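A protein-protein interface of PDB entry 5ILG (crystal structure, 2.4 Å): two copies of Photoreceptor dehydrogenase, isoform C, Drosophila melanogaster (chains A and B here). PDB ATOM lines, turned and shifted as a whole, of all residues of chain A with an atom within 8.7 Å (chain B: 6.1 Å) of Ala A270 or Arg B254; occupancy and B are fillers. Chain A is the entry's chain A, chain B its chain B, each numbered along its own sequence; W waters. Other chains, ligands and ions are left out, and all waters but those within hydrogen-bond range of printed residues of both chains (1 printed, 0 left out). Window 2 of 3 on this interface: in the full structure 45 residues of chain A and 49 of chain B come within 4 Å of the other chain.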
ATOM      1  N   TRP A 264      32.606 -24.604  13.391  1.00  0.00           N
ATOM      2  CA  TRP A 264      31.152 -24.586  13.246  1.00  0.00           C
ATOM      3  C   TRP A 264      30.616 -23.159  13.146  1.00  0.00           C
ATOM      4  O   TRP A 264      30.623 -22.386  14.118  1.00  0.00           O
ATOM      5  CB  TRP A 264      30.480 -25.309  14.429  1.00  0.00           C
ATOM      6  CG  TRP A 264      28.957 -25.232  14.471  1.00  0.00           C
ATOM      7  CD1 TRP A 264      28.155 -25.045  15.589  1.00  0.00           C
ATOM      8  CD2 TRP A 264      28.071 -25.358  13.364  1.00  0.00           C
ATOM      9  NE1 TRP A 264      26.820 -25.041  15.222  1.00  0.00           N
ATOM     10  CE2 TRP A 264      26.742 -25.227  13.866  1.00  0.00           C
ATOM     11  CE3 TRP A 264      28.259 -25.571  11.989  1.00  0.00           C
ATOM     12  CZ2 TRP A 264      25.613 -25.302  13.034  1.00  0.00           C
ATOM     13  CZ3 TRP A 264      27.128 -25.643  11.151  1.00  0.00           C
ATOM     14  CH2 TRP A 264      25.822 -25.503  11.682  1.00  0.00           C
ATOM     15  N   GLY A 266      27.147 -20.936  11.108  1.00  0.00           N
ATOM     16  CA  GLY A 266      25.829 -21.088  10.454  1.00  0.00           C
ATOM     17  C   GLY A 266      25.797 -21.121   8.910  1.00  0.00           C
ATOM     18  O   GLY A 266      24.756 -21.442   8.320  1.00  0.00           O
ATOM     19  N   LYS A 267      26.924 -20.809   8.253  1.00  0.00           N
ATOM     20  CA  LYS A 267      27.022 -20.771   6.767  1.00  0.00           C
ATOM     21  C   LYS A 267      26.746 -22.108   6.055  1.00  0.00           C
ATOM     22  O   LYS A 267      26.269 -22.120   4.913  1.00  0.00           O
ATOM     23  CB  LYS A 267      28.389 -20.237   6.309  1.00  0.00           C
ATOM     24  N   GLU A 268      27.044 -23.220   6.728  1.00  0.00           N
ATOM     25  CA  GLU A 268      26.743 -24.570   6.204  1.00  0.00           C
ATOM     26  C   GLU A 268      25.251 -24.775   5.991  1.00  0.00           C
ATOM     27  O   GLU A 268      24.437 -24.255   6.764  1.00  0.00           O
ATOM     28  CB  GLU A 268      27.246 -25.672   7.139  1.00  0.00           C
ATOM     29  N   GLN A 269      24.922 -25.518   4.931  1.00  0.00           N
ATOM     30  CA  GLN A 269      23.536 -25.900   4.601  1.00  0.00           C
ATOM     31  C   GLN A 269      23.240 -27.298   5.169  1.00  0.00           C
ATOM     32  O   GLN A 269      24.099 -28.191   5.173  1.00  0.00           O
ATOM     33  CB  GLN A 269      23.249 -25.844   3.073  1.00  0.00           C
ATOM     34  CG  GLN A 269      23.361 -24.456   2.421  1.00  0.00           C
ATOM     35  CD  GLN A 269      22.281 -23.451   2.854  1.00  0.00           C
ATOM     36  OE1 GLN A 269      21.074 -23.739   2.777  1.00  0.00           O
ATOM     37  NE2 GLN A 269      22.717 -22.247   3.278  1.00  0.00           N
ATOM     38  N   ALA A 270      22.017 -27.469   5.661  1.00  0.00           N
ATOM     39  CA  ALA A 270      21.563 -28.751   6.185  1.00  0.00           C
ATOM     40  C   ALA A 270      21.485 -29.833   5.072  1.00  0.00           C
ATOM     41  O   ALA A 270      21.045 -29.558   3.959  1.00  0.00           O
ATOM     42  CB  ALA A 270      20.222 -28.575   6.883  1.00  0.00           C
ATOM     43  N   LEU A 271      21.919 -31.054   5.390  1.00  0.00           N
ATOM     44  CA  LEU A 271      22.087 -32.133   4.408  1.00  0.00           C
ATOM     45  C   LEU A 271      22.200 -33.471   5.099  1.00  0.00           C
ATOM     46  O   LEU A 271      23.195 -34.174   4.903  1.00  0.00           O
ATOM     47  CB  LEU A 271      23.367 -31.917   3.576  1.00  0.00           C
ATOM     48  N   GLN B 226      17.101 -30.815  20.698  1.00  0.00           N
ATOM     49  CA  GLN B 226      17.097 -32.053  19.911  1.00  0.00           C
ATOM     50  C   GLN B 226      17.174 -33.257  20.825  1.00  0.00           C
ATOM     51  O   GLN B 226      17.738 -33.194  21.901  1.00  0.00           O
ATOM     52  CB  GLN B 226      18.211 -32.090  18.844  1.00  0.00           C
ATOM     53  CG  GLN B 226      19.606 -32.310  19.382  1.00  0.00           C
ATOM     54  CD  GLN B 226      20.706 -32.074  18.358  1.00  0.00           C
ATOM     55  OE1 GLN B 226      20.475 -31.721  17.188  1.00  0.00           O
ATOM     56  NE2 GLN B 226      21.930 -32.258  18.795  1.00  0.00           N
ATOM     57  N   CYS B 234      19.696 -38.285  12.155  1.00  0.00           N
ATOM     58  CA  CYS B 234      20.805 -37.615  11.474  1.00  0.00           C
ATOM     59  C   CYS B 234      21.993 -38.543  11.219  1.00  0.00           C
ATOM     60  O   CYS B 234      22.658 -38.455  10.187  1.00  0.00           O
ATOM     61  CB  CYS B 234      21.250 -36.409  12.287  1.00  0.00           C
ATOM     62  SG  CYS B 234      20.067 -35.032  12.229  1.00  0.00           S
ATOM     63  N   VAL B 249      28.239 -31.744  11.675  1.00  0.00           N
ATOM     64  CA  VAL B 249      27.678 -31.161  12.895  1.00  0.00           C
ATOM     65  C   VAL B 249      26.193 -31.511  12.958  1.00  0.00           C
ATOM     66  O   VAL B 249      25.483 -31.415  11.951  1.00  0.00           O
ATOM     67  CB  VAL B 249      27.897 -29.651  12.959  1.00  0.00           C
ATOM     68  CG1 VAL B 249      27.058 -29.013  14.043  1.00  0.00           C
ATOM     69  CG2 VAL B 249      29.362 -29.349  13.202  1.00  0.00           C
ATOM     70  N   ILE B 250      25.732 -31.924  14.133  1.00  0.00           N
ATOM     71  CA  ILE B 250      24.312 -32.266  14.313  1.00  0.00           C
ATOM     72  C   ILE B 250      23.738 -31.322  15.338  1.00  0.00           C
ATOM     73  O   ILE B 250      23.969 -31.478  16.534  1.00  0.00           O
ATOM     74  CB  ILE B 250      24.065 -33.742  14.688  1.00  0.00           C
ATOM     75  CG1 ILE B 250      24.652 -34.677  13.618  1.00  0.00           C
ATOM     76  CG2 ILE B 250      22.572 -34.031  14.812  1.00  0.00           C
ATOM     77  CD1 ILE B 250      24.666 -36.145  14.000  1.00  0.00           C
ATOM     78  N   GLU B 251      22.963 -30.354  14.854  1.00  0.00           N
ATOM     79  CA  GLU B 251      22.377 -29.294  15.693  1.00  0.00           C
ATOM     80  C   GLU B 251      20.955 -28.999  15.273  1.00  0.00           C
ATOM     81  O   GLU B 251      20.642 -28.975  14.099  1.00  0.00           O
ATOM     82  CB  GLU B 251      23.211 -28.030  15.576  1.00  0.00           C
ATOM     83  CG  GLU B 251      22.885 -26.989  16.639  1.00  0.00           C
ATOM     84  CD  GLU B 251      23.704 -27.162  17.900  1.00  0.00           C
ATOM     85  OE1 GLU B 251      24.903 -27.513  17.787  1.00  0.00           O
ATOM     86  OE2 GLU B 251      23.146 -26.925  18.990  1.00  0.00           O
ATOM     87  N   GLY B 252      20.093 -28.773  16.251  1.00  0.00           N
ATOM     88  CA  GLY B 252      18.676 -28.523  15.996  1.00  0.00           C
ATOM     89  C   GLY B 252      18.060 -29.527  15.036  1.00  0.00           C
ATOM     90  O   GLY B 252      17.364 -29.162  14.107  1.00  0.00           O
ATOM     91  N   LYS B 253      18.355 -30.801  15.272  1.00  0.00           N
ATOM     92  CA  LYS B 253      17.785 -31.940  14.523  1.00  0.00           C
ATOM     93  C   LYS B 253      18.237 -32.055  13.076  1.00  0.00           C
ATOM     94  O   LYS B 253      17.705 -32.861  12.320  1.00  0.00           O
ATOM     95  CB  LYS B 253      16.258 -31.904  14.569  1.00  0.00           C
ATOM     96  CG  LYS B 253      15.676 -31.668  15.953  1.00  0.00           C
ATOM     97  CD  LYS B 253      14.175 -31.450  15.834  1.00  0.00           C
ATOM     98  CE  LYS B 253      13.528 -31.233  17.179  1.00  0.00           C
ATOM     99  NZ  LYS B 253      12.062 -31.346  17.021  1.00  0.00           N
ATOM    100  N   ARG B 254      19.246 -31.287  12.707  1.00  0.00           N
ATOM    101  CA  ARG B 254      19.725 -31.250  11.342  1.00  0.00           C
ATOM    102  C   ARG B 254      21.202 -31.566  11.196  1.00  0.00           C
ATOM    103  O   ARG B 254      21.995 -31.331  12.102  1.00  0.00           O
ATOM    104  CB  ARG B 254      19.428 -29.881  10.756  1.00  0.00           C
ATOM    105  CG  ARG B 254      17.930 -29.595  10.713  1.00  0.00           C
ATOM    106  CD  ARG B 254      17.489 -28.940   9.412  1.00  0.00           C
ATOM    107  NE  ARG B 254      16.928 -29.902   8.471  1.00  0.00           N
ATOM    108  CZ  ARG B 254      16.639 -29.630   7.205  1.00  0.00           C
ATOM    109  NH1 ARG B 254      16.110 -30.581   6.429  1.00  0.00           N
ATOM    110  NH2 ARG B 254      16.878 -28.415   6.709  1.00  0.00           N
ATOM    111  N   VAL B 255      21.566 -32.077  10.031  1.00  0.00           N
ATOM    112  CA  VAL B 255      22.950 -32.461   9.735  1.00  0.00           C
ATOM    113  C   VAL B 255      23.641 -31.406   8.907  1.00  0.00           C
ATOM    114  O   VAL B 255      23.164 -31.077   7.827  1.00  0.00           O
ATOM    115  CB  VAL B 255      23.043 -33.745   8.899  1.00  0.00           C
ATOM    116  CG1 VAL B 255      24.487 -34.210   8.843  1.00  0.00           C
ATOM    117  CG2 VAL B 255      22.224 -34.836   9.490  1.00  0.00           C
ATOM    118  N   TYR B 256      24.795 -30.940   9.373  1.00  0.00           N
ATOM    119  CA  TYR B 256      25.567 -29.906   8.652  1.00  0.00           C
ATOM    120  C   TYR B 256      26.966 -30.426   8.286  1.00  0.00           C
ATOM    121  O   TYR B 256      27.797 -30.638   9.154  1.00  0.00           O
ATOM    122  CB  TYR B 256      25.678 -28.610   9.458  1.00  0.00           C
ATOM    123  CG  TYR B 256      24.364 -27.933   9.838  1.00  0.00           C
ATOM    124  CD1 TYR B 256      23.593 -28.420  10.891  1.00  0.00           C
ATOM    125  CD2 TYR B 256      23.925 -26.771   9.196  1.00  0.00           C
ATOM    126  CE1 TYR B 256      22.414 -27.801  11.274  1.00  0.00           C
ATOM    127  CE2 TYR B 256      22.746 -26.133   9.582  1.00  0.00           C
ATOM    128  CZ  TYR B 256      21.991 -26.663  10.612  1.00  0.00           C
ATOM    129  OH  TYR B 256      20.816 -26.095  10.996  1.00  0.00           O
ATOM    130  N   PRO B 257      27.225 -30.666   6.996  1.00  0.00           N
ATOM    131  CA  PRO B 257      28.532 -31.112   6.535  1.00  0.00           C
ATOM    132  C   PRO B 257      29.558 -30.025   6.672  1.00  0.00           C
ATOM    133  O   PRO B 257      29.311 -28.923   6.255  1.00  0.00           O
ATOM    134  CB  PRO B 257      28.320 -31.417   5.045  1.00  0.00           C
ATOM    135  CG  PRO B 257      26.858 -31.517   4.875  1.00  0.00           C
ATOM    136  CD  PRO B 257      26.273 -30.592   5.886  1.00  0.00           C
HETATM  137  O   HOH W   1      19.034 -31.664   5.654  1.00  0.00           O
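Water W1 lies within hydrogen-bond range of the backbone NH of Leu A271, the guanidinium group of Arg B254 and the backbone carbonyl oxygen of Ala A270.
No position is printed for both chains.
Of the 9 pairs that touch across the chains among the printed residues, none has its exchanged pair printed and touching as well.
Of the printed residues of chain B, Trp A264 touches Val B249 (3.8 Å) and Tyr B256 (3.4 Å).
Ala A270 touches two residues of chain B.
Of the printed residues of chain A, Val B249 touches Trp A264.
No residue of chain A comes within 4 Å of Gly B252.
Arg B254 touches one residue of chain A.
Of the printed residues of chain A, Val B255 touches Ala A270 (3.3 Å) and Leu A271 (2.7 Å).
Of the printed residues of chain A, Tyr B256 touches Trp A264 (3.4 Å) and Glu A268 (3.5 Å).
Of the 7 printed residues of chain A, 5 touch a printed residue of chain B.
Hydrophobic or aromatic side chains of chain A that line the printed part of chain B: Trp A264, Ala A270 and Leu A271.
Of the 11 printed residues of chain B, 5 touch a printed residue of chain A.
Hydrophobic or aromatic side chains of chain B within 4 Å of the printed part of chain A: Val B249, Val B255, Tyr B256 and Pro B257.
Among the printed residues, 9 pairs touch across the chains.
Among the printed residues, merely in contact across the chains: Ala A270 with Val B255 (3.3 Å), Gln A269 with Pro B257 (3.3 Å), Ala A270 with Arg B254 (3.4 Å), Trp A264 with Tyr B256 (3.4 Å), Glu A268 with Tyr B256 (3.5 Å), Leu A271 with Pro B257 (3.7 Å), Trp A264 with Val B249 (3.8 Å) and Glu A268 with Pro B257 (3.95 Å).
N of Leu A271 sits at hydrogen-bond distance from O of Val B255 (2.7 Å).
The backbone NH of Tyr B256 lies within hydrogen-bond range of the backbone carbonyl oxygen of Val B249, 2.7 Å away.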
